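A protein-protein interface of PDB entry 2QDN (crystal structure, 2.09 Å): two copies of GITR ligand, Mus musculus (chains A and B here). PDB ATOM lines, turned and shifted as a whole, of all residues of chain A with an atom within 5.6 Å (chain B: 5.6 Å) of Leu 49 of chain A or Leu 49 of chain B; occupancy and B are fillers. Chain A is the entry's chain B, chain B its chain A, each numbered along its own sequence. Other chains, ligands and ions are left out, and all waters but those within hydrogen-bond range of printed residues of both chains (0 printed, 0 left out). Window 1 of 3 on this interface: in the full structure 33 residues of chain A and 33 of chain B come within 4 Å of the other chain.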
ATOM      1  N   MET A  12     -24.540 -21.089  13.704  1.00  0.00           N
ATOM      2  CA  MET A  12     -24.462 -20.890  15.142  1.00  0.00           C
ATOM      3  C   MET A  12     -24.475 -22.229  15.855  1.00  0.00           C
ATOM      4  O   MET A  12     -25.253 -23.128  15.484  1.00  0.00           O
ATOM      5  CB  MET A  12     -25.633 -20.036  15.650  1.00  0.00           C
ATOM      6  CG  MET A  12     -25.599 -19.799  17.160  1.00  0.00           C
ATOM      7  SD  MET A  12     -26.866 -18.621  17.723  1.00  0.00           S
ATOM      8  CE  MET A  12     -26.332 -18.284  19.403  1.00  0.00           C
ATOM      9  N   THR A  47     -15.840 -12.939  10.779  1.00  0.00           N
ATOM     10  CA  THR A  47     -16.100 -12.231  12.014  1.00  0.00           C
ATOM     11  C   THR A  47     -17.097 -13.065  12.796  1.00  0.00           C
ATOM     12  O   THR A  47     -18.143 -13.396  12.276  1.00  0.00           O
ATOM     13  CB  THR A  47     -16.761 -10.883  11.709  1.00  0.00           C
ATOM     14  OG1 THR A  47     -15.995 -10.240  10.690  1.00  0.00           O
ATOM     15  CG2 THR A  47     -16.829  -9.995  12.980  1.00  0.00           C
ATOM     16  N   TYR A  48     -16.760 -13.376  14.035  1.00  0.00           N
ATOM     17  CA  TYR A  48     -17.560 -14.264  14.873  1.00  0.00           C
ATOM     18  C   TYR A  48     -17.874 -13.583  16.173  1.00  0.00           C
ATOM     19  O   TYR A  48     -17.086 -12.803  16.690  1.00  0.00           O
ATOM     20  CB  TYR A  48     -16.802 -15.562  15.196  1.00  0.00           C
ATOM     21  CG  TYR A  48     -16.743 -16.540  14.037  1.00  0.00           C
ATOM     22  CD1 TYR A  48     -17.662 -17.579  13.946  1.00  0.00           C
ATOM     23  CD2 TYR A  48     -15.780 -16.420  13.026  1.00  0.00           C
ATOM     24  CE1 TYR A  48     -17.640 -18.485  12.901  1.00  0.00           C
ATOM     25  CE2 TYR A  48     -15.743 -17.341  11.953  1.00  0.00           C
ATOM     26  CZ  TYR A  48     -16.673 -18.368  11.914  1.00  0.00           C
ATOM     27  OH  TYR A  48     -16.686 -19.293  10.906  1.00  0.00           O
ATOM     28  N   LEU A  49     -19.039 -13.905  16.713  1.00  0.00           N
ATOM     29  CA  LEU A  49     -19.312 -13.558  18.068  1.00  0.00           C
ATOM     30  C   LEU A  49     -19.137 -14.818  18.883  1.00  0.00           C
ATOM     31  O   LEU A  49     -19.853 -15.808  18.661  1.00  0.00           O
ATOM     32  CB  LEU A  49     -20.742 -13.012  18.175  1.00  0.00           C
ATOM     33  CG  LEU A  49     -21.278 -12.653  19.561  1.00  0.00           C
ATOM     34  CD1 LEU A  49     -20.454 -11.537  20.190  1.00  0.00           C
ATOM     35  CD2 LEU A  49     -22.736 -12.230  19.338  1.00  0.00           C
ATOM     36  N   ILE A  50     -18.171 -14.781  19.806  1.00  0.00           N
ATOM     37  CA  ILE A  50     -17.948 -15.821  20.797  1.00  0.00           C
ATOM     38  C   ILE A  50     -18.732 -15.377  22.017  1.00  0.00           C
ATOM     39  O   ILE A  50     -18.631 -14.223  22.411  1.00  0.00           O
ATOM     40  CB  ILE A  50     -16.427 -15.961  21.190  1.00  0.00           C
ATOM     41  CG1 ILE A  50     -15.528 -16.221  19.964  1.00  0.00           C
ATOM     42  CG2 ILE A  50     -16.203 -17.004  22.295  1.00  0.00           C
ATOM     43  CD1 ILE A  50     -13.986 -16.274  20.326  1.00  0.00           C
ATOM     44  N   TYR A  51     -19.506 -16.292  22.613  1.00  0.00           N
ATOM     45  CA  TYR A  51     -20.417 -15.937  23.704  1.00  0.00           C
ATOM     46  C   TYR A  51     -20.513 -17.096  24.696  1.00  0.00           C
ATOM     47  O   TYR A  51     -20.038 -18.203  24.447  1.00  0.00           O
ATOM     48  CB  TYR A  51     -21.821 -15.584  23.139  1.00  0.00           C
ATOM     49  CG  TYR A  51     -22.539 -16.831  22.619  1.00  0.00           C
ATOM     50  CD1 TYR A  51     -23.454 -17.528  23.426  1.00  0.00           C
ATOM     51  CD2 TYR A  51     -22.276 -17.325  21.323  1.00  0.00           C
ATOM     52  CE1 TYR A  51     -24.105 -18.676  22.953  1.00  0.00           C
ATOM     53  CE2 TYR A  51     -22.901 -18.464  20.851  1.00  0.00           C
ATOM     54  CZ  TYR A  51     -23.803 -19.144  21.671  1.00  0.00           C
ATOM     55  OH  TYR A  51     -24.398 -20.281  21.193  1.00  0.00           O
ATOM     56  N   GLY A  92     -16.606 -13.754  26.050  1.00  0.00           N
ATOM     57  CA  GLY A  92     -16.586 -13.556  24.598  1.00  0.00           C
ATOM     58  C   GLY A  92     -16.610 -12.119  24.135  1.00  0.00           C
ATOM     59  O   GLY A  92     -16.175 -11.217  24.856  1.00  0.00           O
ATOM     60  N   GLY A  93     -17.115 -11.919  22.918  1.00  0.00           N
ATOM     61  CA  GLY A  93     -17.073 -10.646  22.234  1.00  0.00           C
ATOM     62  C   GLY A  93     -16.907 -10.944  20.753  1.00  0.00           C
ATOM     63  O   GLY A  93     -16.950 -12.102  20.359  1.00  0.00           O
ATOM     64  N   VAL A  94     -16.728  -9.895  19.951  1.00  0.00           N
ATOM     65  CA  VAL A  94     -16.568 -10.000  18.518  1.00  0.00           C
ATOM     66  C   VAL A  94     -15.074 -10.159  18.198  1.00  0.00           C
ATOM     67  O   VAL A  94     -14.246  -9.362  18.660  1.00  0.00           O
ATOM     68  CB  VAL A  94     -17.195  -8.753  17.800  1.00  0.00           C
ATOM     69  CG1 VAL A  94     -16.861  -8.742  16.342  1.00  0.00           C
ATOM     70  CG2 VAL A  94     -18.729  -8.725  18.010  1.00  0.00           C
ATOM     71  N   TYR A  95     -14.759 -11.226  17.451  1.00  0.00           N
ATOM     72  CA  TYR A  95     -13.392 -11.598  17.051  1.00  0.00           C
ATOM     73  C   TYR A  95     -13.330 -12.034  15.573  1.00  0.00           C
ATOM     74  O   TYR A  95     -14.233 -12.731  15.073  1.00  0.00           O
ATOM     75  CB  TYR A  95     -12.836 -12.730  17.953  1.00  0.00           C
ATOM     76  CG  TYR A  95     -12.716 -12.315  19.405  1.00  0.00           C
ATOM     77  CD1 TYR A  95     -11.571 -11.644  19.876  1.00  0.00           C
ATOM     78  CD2 TYR A  95     -13.759 -12.552  20.303  1.00  0.00           C
ATOM     79  CE1 TYR A  95     -11.483 -11.214  21.221  1.00  0.00           C
ATOM     80  CE2 TYR A  95     -13.680 -12.140  21.637  1.00  0.00           C
ATOM     81  CZ  TYR A  95     -12.545 -11.477  22.088  1.00  0.00           C
ATOM     82  OH  TYR A  95     -12.498 -11.078  23.409  1.00  0.00           O
ATOM     83  N   GLY A 121     -20.483 -20.848  22.907  1.00  0.00           N
ATOM     84  CA  GLY A 121     -20.503 -21.166  21.498  1.00  0.00           C
ATOM     85  C   GLY A 121     -20.052 -20.009  20.637  1.00  0.00           C
ATOM     86  O   GLY A 121     -19.462 -19.061  21.125  1.00  0.00           O
ATOM     87  N   ILE A 122     -20.311 -20.122  19.342  1.00  0.00           N
ATOM     88  CA  ILE A 122     -20.019 -19.057  18.404  1.00  0.00           C
ATOM     89  C   ILE A 122     -21.192 -18.877  17.475  1.00  0.00           C
ATOM     90  O   ILE A 122     -22.053 -19.747  17.363  1.00  0.00           O
ATOM     91  CB  ILE A 122     -18.715 -19.291  17.531  1.00  0.00           C
ATOM     92  CG1 ILE A 122     -18.689 -20.645  16.833  1.00  0.00           C
ATOM     93  CG2 ILE A 122     -17.460 -19.138  18.358  1.00  0.00           C
ATOM     94  CD1 ILE A 122     -19.546 -20.708  15.572  1.00  0.00           C
ATOM     95  N   ILE A 123     -21.211 -17.724  16.833  1.00  0.00           N
ATOM     96  CA  ILE A 123     -22.061 -17.484  15.702  1.00  0.00           C
ATOM     97  C   ILE A 123     -21.239 -16.677  14.705  1.00  0.00           C
ATOM     98  O   ILE A 123     -20.534 -15.723  15.085  1.00  0.00           O
ATOM     99  CB  ILE A 123     -23.414 -16.769  16.087  1.00  0.00           C
ATOM    100  CG1 ILE A 123     -24.226 -16.401  14.835  1.00  0.00           C
ATOM    101  CG2 ILE A 123     -23.189 -15.569  16.963  1.00  0.00           C
ATOM    102  CD1 ILE A 123     -25.725 -16.142  15.084  1.00  0.00           C
ATOM    103  N   LEU A 124     -21.283 -17.127  13.451  1.00  0.00           N
ATOM    104  CA  LEU A 124     -20.715 -16.392  12.350  1.00  0.00           C
ATOM    105  C   LEU A 124     -21.619 -15.180  12.086  1.00  0.00           C
ATOM    106  O   LEU A 124     -22.823 -15.336  11.798  1.00  0.00           O
ATOM    107  CB  LEU A 124     -20.598 -17.296  11.105  1.00  0.00           C
ATOM    108  CG  LEU A 124     -20.180 -16.612   9.800  1.00  0.00           C
ATOM    109  CD1 LEU A 124     -18.773 -16.020   9.904  1.00  0.00           C
ATOM    110  CD2 LEU A 124     -20.295 -17.594   8.631  1.00  0.00           C
ATOM    111  N   MET A 125     -21.039 -13.990  12.225  1.00  0.00           N
ATOM    112  CA  MET A 125     -21.795 -12.743  12.091  1.00  0.00           C
ATOM    113  C   MET A 125     -22.060 -12.354  10.638  1.00  0.00           C
ATOM    114  O   MET A 125     -21.203 -12.516   9.791  1.00  0.00           O
ATOM    115  CB  MET A 125     -21.067 -11.586  12.776  1.00  0.00           C
ATOM    116  CG  MET A 125     -21.253 -11.575  14.272  1.00  0.00           C
ATOM    117  SD  MET A 125     -20.055 -10.555  15.124  1.00  0.00           S
ATOM    118  CE  MET A 125     -20.191  -8.941  14.285  1.00  0.00           C
ATOM    119  N   MET B  12     -29.179  -8.166  13.102  1.00  0.00           N
ATOM    120  CA  MET B  12     -28.164  -7.898  14.117  1.00  0.00           C
ATOM    121  C   MET B  12     -27.779  -6.434  14.094  1.00  0.00           C
ATOM    122  O   MET B  12     -27.700  -5.814  13.025  1.00  0.00           O
ATOM    123  CB  MET B  12     -26.932  -8.779  13.893  1.00  0.00           C
ATOM    124  CG  MET B  12     -25.806  -8.504  14.887  1.00  0.00           C
ATOM    125  SD  MET B  12     -24.284  -9.414  14.581  1.00  0.00           S
ATOM    126  CE  MET B  12     -23.460  -9.205  16.170  1.00  0.00           C
ATOM    127  N   THR B  47     -35.705 -15.476  20.476  1.00  0.00           N
ATOM    128  CA  THR B  47     -34.500 -15.742  21.254  1.00  0.00           C
ATOM    129  C   THR B  47     -33.359 -14.855  20.724  1.00  0.00           C
ATOM    130  O   THR B  47     -33.050 -14.849  19.529  1.00  0.00           O
ATOM    131  CB  THR B  47     -34.146 -17.245  21.157  1.00  0.00           C
ATOM    132  OG1 THR B  47     -35.297 -17.992  21.569  1.00  0.00           O
ATOM    133  CG2 THR B  47     -32.967 -17.619  22.067  1.00  0.00           C
ATOM    134  N   TYR B  48     -32.770 -14.088  21.628  1.00  0.00           N
ATOM    135  CA  TYR B  48     -31.788 -13.102  21.255  1.00  0.00           C
ATOM    136  C   TYR B  48     -30.509 -13.394  22.009  1.00  0.00           C
ATOM    137  O   TYR B  48     -30.524 -13.859  23.144  1.00  0.00           O
ATOM    138  CB  TYR B  48     -32.263 -11.685  21.593  1.00  0.00           C
ATOM    139  CG  TYR B  48     -33.308 -11.161  20.627  1.00  0.00           C
ATOM    140  CD1 TYR B  48     -32.923 -10.438  19.491  1.00  0.00           C
ATOM    141  CD2 TYR B  48     -34.670 -11.417  20.827  1.00  0.00           C
ATOM    142  CE1 TYR B  48     -33.870  -9.963  18.572  1.00  0.00           C
ATOM    143  CE2 TYR B  48     -35.640 -10.933  19.913  1.00  0.00           C
ATOM    144  CZ  TYR B  48     -35.222 -10.195  18.789  1.00  0.00           C
ATOM    145  OH  TYR B  48     -36.130  -9.715  17.859  1.00  0.00           O
ATOM    146  N   LEU B  49     -29.414 -13.132  21.338  1.00  0.00           N
ATOM    147  CA  LEU B  49     -28.128 -13.059  21.985  1.00  0.00           C
ATOM    148  C   LEU B  49     -27.804 -11.574  22.175  1.00  0.00           C
ATOM    149  O   LEU B  49     -27.626 -10.845  21.203  1.00  0.00           O
ATOM    150  CB  LEU B  49     -27.079 -13.787  21.145  1.00  0.00           C
ATOM    151  CG  LEU B  49     -25.626 -13.836  21.658  1.00  0.00           C
ATOM    152  CD1 LEU B  49     -25.541 -14.361  23.088  1.00  0.00           C
ATOM    153  CD2 LEU B  49     -24.812 -14.724  20.719  1.00  0.00           C
ATOM    154  N   ILE B  50     -27.773 -11.153  23.438  1.00  0.00           N
ATOM    155  CA  ILE B  50     -27.326  -9.831  23.866  1.00  0.00           C
ATOM    156  C   ILE B  50     -25.839  -9.980  24.160  1.00  0.00           C
ATOM    157  O   ILE B  50     -25.406 -10.954  24.814  1.00  0.00           O
ATOM    158  CB  ILE B  50     -28.102  -9.332  25.147  1.00  0.00           C
ATOM    159  CG1 ILE B  50     -29.623  -9.376  24.910  1.00  0.00           C
ATOM    160  CG2 ILE B  50     -27.608  -7.944  25.603  1.00  0.00           C
ATOM    161  CD1 ILE B  50     -30.491  -8.976  26.206  1.00  0.00           C
ATOM    162  N   TYR B  51     -25.055  -9.030  23.642  1.00  0.00           N
ATOM    163  CA  TYR B  51     -23.610  -9.117  23.724  1.00  0.00           C
ATOM    164  C   TYR B  51     -23.045  -7.708  23.913  1.00  0.00           C
ATOM    165  O   TYR B  51     -23.791  -6.707  23.848  1.00  0.00           O
ATOM    166  CB  TYR B  51     -23.031  -9.802  22.461  1.00  0.00           C
ATOM    167  CG  TYR B  51     -23.157  -8.939  21.238  1.00  0.00           C
ATOM    168  CD1 TYR B  51     -22.108  -8.092  20.841  1.00  0.00           C
ATOM    169  CD2 TYR B  51     -24.346  -8.920  20.489  1.00  0.00           C
ATOM    170  CE1 TYR B  51     -22.257  -7.267  19.711  1.00  0.00           C
ATOM    171  CE2 TYR B  51     -24.496  -8.105  19.382  1.00  0.00           C
ATOM    172  CZ  TYR B  51     -23.457  -7.270  19.005  1.00  0.00           C
ATOM    173  OH  TYR B  51     -23.627  -6.469  17.899  1.00  0.00           O
ATOM    174  N   GLY B  92     -23.935  -9.985  28.657  1.00  0.00           N
ATOM    175  CA  GLY B  92     -25.075 -10.527  27.919  1.00  0.00           C
ATOM    176  C   GLY B  92     -25.175 -12.043  27.998  1.00  0.00           C
ATOM    177  O   GLY B  92     -24.684 -12.664  28.923  1.00  0.00           O
ATOM    178  N   GLY B  93     -25.769 -12.634  26.974  1.00  0.00           N
ATOM    179  CA  GLY B  93     -26.130 -14.042  27.008  1.00  0.00           C
ATOM    180  C   GLY B  93     -27.391 -14.215  26.191  1.00  0.00           C
ATOM    181  O   GLY B  93     -27.904 -13.255  25.611  1.00  0.00           O
ATOM    182  N   VAL B  94     -27.883 -15.448  26.159  1.00  0.00           N
ATOM    183  CA  VAL B  94     -29.081 -15.822  25.439  1.00  0.00           C
ATOM    184  C   VAL B  94     -30.304 -15.557  26.315  1.00  0.00           C
ATOM    185  O   VAL B  94     -30.388 -16.061  27.441  1.00  0.00           O
ATOM    186  CB  VAL B  94     -29.024 -17.334  25.049  1.00  0.00           C
ATOM    187  CG1 VAL B  94     -30.342 -17.781  24.412  1.00  0.00           C
ATOM    188  CG2 VAL B  94     -27.849 -17.607  24.124  1.00  0.00           C
ATOM    189  N   TYR B  95     -31.233 -14.742  25.808  1.00  0.00           N
ATOM    190  CA  TYR B  95     -32.463 -14.382  26.510  1.00  0.00           C
ATOM    191  C   TYR B  95     -33.658 -14.487  25.547  1.00  0.00           C
ATOM    192  O   TYR B  95     -33.544 -14.146  24.378  1.00  0.00           O
ATOM    193  CB  TYR B  95     -32.363 -12.961  27.130  1.00  0.00           C
ATOM    194  CG  TYR B  95     -31.296 -12.871  28.211  1.00  0.00           C
ATOM    195  CD1 TYR B  95     -31.592 -13.181  29.557  1.00  0.00           C
ATOM    196  CD2 TYR B  95     -29.993 -12.526  27.893  1.00  0.00           C
ATOM    197  CE1 TYR B  95     -30.598 -13.120  30.549  1.00  0.00           C
ATOM    198  CE2 TYR B  95     -28.992 -12.462  28.876  1.00  0.00           C
ATOM    199  CZ  TYR B  95     -29.298 -12.748  30.184  1.00  0.00           C
ATOM    200  OH  TYR B  95     -28.300 -12.686  31.129  1.00  0.00           O
ATOM    201  N   GLY B 121     -24.852  -4.890  21.698  1.00  0.00           N
ATOM    202  CA  GLY B 121     -25.939  -5.009  20.723  1.00  0.00           C
ATOM    203  C   GLY B 121     -26.701  -6.281  20.936  1.00  0.00           C
ATOM    204  O   GLY B 121     -26.582  -6.892  21.997  1.00  0.00           O
ATOM    205  N   ILE B 122     -27.502  -6.657  19.940  1.00  0.00           N
ATOM    206  CA  ILE B 122     -28.233  -7.921  19.956  1.00  0.00           C
ATOM    207  C   ILE B 122     -28.196  -8.524  18.597  1.00  0.00           C
ATOM    208  O   ILE B 122     -28.056  -7.829  17.593  1.00  0.00           O
ATOM    209  CB  ILE B 122     -29.766  -7.817  20.273  1.00  0.00           C
ATOM    210  CG1 ILE B 122     -30.444  -6.758  19.407  1.00  0.00           C
ATOM    211  CG2 ILE B 122     -30.033  -7.653  21.751  1.00  0.00           C
ATOM    212  CD1 ILE B 122     -31.906  -6.930  19.303  1.00  0.00           C
ATOM    213  N   ILE B 123     -28.370  -9.833  18.584  1.00  0.00           N
ATOM    214  CA  ILE B 123     -28.644 -10.557  17.363  1.00  0.00           C
ATOM    215  C   ILE B 123     -29.837 -11.489  17.584  1.00  0.00           C
ATOM    216  O   ILE B 123     -29.909 -12.180  18.611  1.00  0.00           O
ATOM    217  CB  ILE B 123     -27.377 -11.321  16.839  1.00  0.00           C
ATOM    218  CG1 ILE B 123     -27.745 -12.315  15.719  1.00  0.00           C
ATOM    219  CG2 ILE B 123     -26.652 -12.029  17.954  1.00  0.00           C
ATOM    220  CD1 ILE B 123     -26.579 -12.567  14.748  1.00  0.00           C
ATOM    221  N   LEU B 124     -30.773 -11.471  16.630  1.00  0.00           N
ATOM    222  CA  LEU B 124     -31.873 -12.425  16.601  1.00  0.00           C
ATOM    223  C   LEU B 124     -31.310 -13.760  16.198  1.00  0.00           C
ATOM    224  O   LEU B 124     -30.757 -13.919  15.093  1.00  0.00           O
ATOM    225  CB  LEU B 124     -32.988 -11.987  15.651  1.00  0.00           C
ATOM    226  CG  LEU B 124     -34.192 -12.922  15.429  1.00  0.00           C
ATOM    227  CD1 LEU B 124     -35.053 -13.188  16.679  1.00  0.00           C
ATOM    228  CD2 LEU B 124     -35.057 -12.378  14.285  1.00  0.00           C
ATOM    229  N   MET B 125     -31.439 -14.723  17.109  1.00  0.00           N
ATOM    230  CA  MET B 125     -30.858 -16.041  16.913  1.00  0.00           C
ATOM    231  C   MET B 125     -31.650 -16.905  15.931  1.00  0.00           C
ATOM    232  O   MET B 125     -32.880 -16.874  15.921  1.00  0.00           O
ATOM    233  CB  MET B 125     -30.702 -16.762  18.266  1.00  0.00           C
ATOM    234  CG  MET B 125     -29.492 -16.295  19.034  1.00  0.00           C
ATOM    235  SD  MET B 125     -29.432 -16.896  20.736  1.00  0.00           S
ATOM    236  CE  MET B 125     -29.667 -18.681  20.541  1.00  0.00           C
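O of Thr 47 of chain B is in hydrogen-bond range of N of Met 125 of chain B, at 2.9 Å.
The backbone carbonyl oxygen (O) of Tyr 51 of chain A sits at hydrogen-bond distance from the backbone NH (N) of Gly 121 of chain A (3.1 Å).
The backbone carbonyl oxygen (O) of Leu 49 of chain B lies within hydrogen-bond range of the backbone NH (N) of Ile 123 of chain B (2.9 Å).
The backbone carbonyl oxygen of Thr 47 of chain A sits at hydrogen-bond distance from the backbone NH of Met 125 of chain A, 3.0 Å away.
O of Tyr 51 of chain B lies within hydrogen-bond range of N of Gly 121 of chain B (3.0 Å).
The backbone carbonyl oxygen (O) of Ile 123 of chain A lies within hydrogen-bond range of the backbone NH (N) of Leu 49 of chain A (2.9 Å).
Met 125 of chain B touches Met 12 of chain A.
Leu 49 of chain B touches Leu 49 of chain A.
CD2 of Leu 49 of chain A touches CG of Tyr 51 of chain B, 3.8 Å away.
CD2 of Leu 49 of chain B touches CG of Tyr 51 of chain A, at 3.6 Å.
Ile 123 of chain A touches Ile 123 of chain B.
Met 12 of chain B touches Met 125 of chain A.
Printed residues of chain B within 4 Å of Met 12 of chain A: Met 125 (3.5 Å).
Leu 49 of chain A touches just these residues of chain B: Leu 49 and Tyr 51.
Val 94 of chain A touches none of the printed residues of chain B.
Leu 49 of chain B touches two residues of chain A.
Of the printed residues of chain A, Met 125 of chain B touches Met 12 (3.5 Å).
The nearest residue of chain B that does not touch Leu 49 of chain A is Ile 123 of chain B (4.2 Å).
Of the 15 printed residues of chain B, 5 touch a printed residue of chain A.
Printed residues of chain B that touch a printed residue of chain A: Met 12, Leu 49, Tyr 51, Ile 123 and Met 125.
Along chain B the printed residues that touch a printed residue of chain A span positions 12 to 125.
Of the 15 printed residues of chain A, 5 touch a printed residue of chain B.
Printed residues of chain A that touch a printed residue of chain B: Met 12, Leu 49, Tyr 51, Ile 123 and Met 125.
Among the printed residues, no Asp or Glu carboxylate lies within 4 Å of a Lys or Arg side-chain nitrogen of the other chain.
Met 12 of chain A touches Met 125 of chain B, and with the chains exchanged Met 125 of chain A touches Met 12 of chain B.
Leu 49 of chain B touches its own counterpart, Leu 49 of chain A.
Leu 49 of chain A touches Tyr 51 of chain B, and with the chains exchanged Tyr 51 of chain A touches Leu 49 of chain B.
Ile 123 of chain B touches its own counterpart, Ile 123 of chain A.
Positions printed for both chains: 12, 47, 48, 49, 50, 51, 92, 93, 94, 95, 121, 122, 123, 124 and 125.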
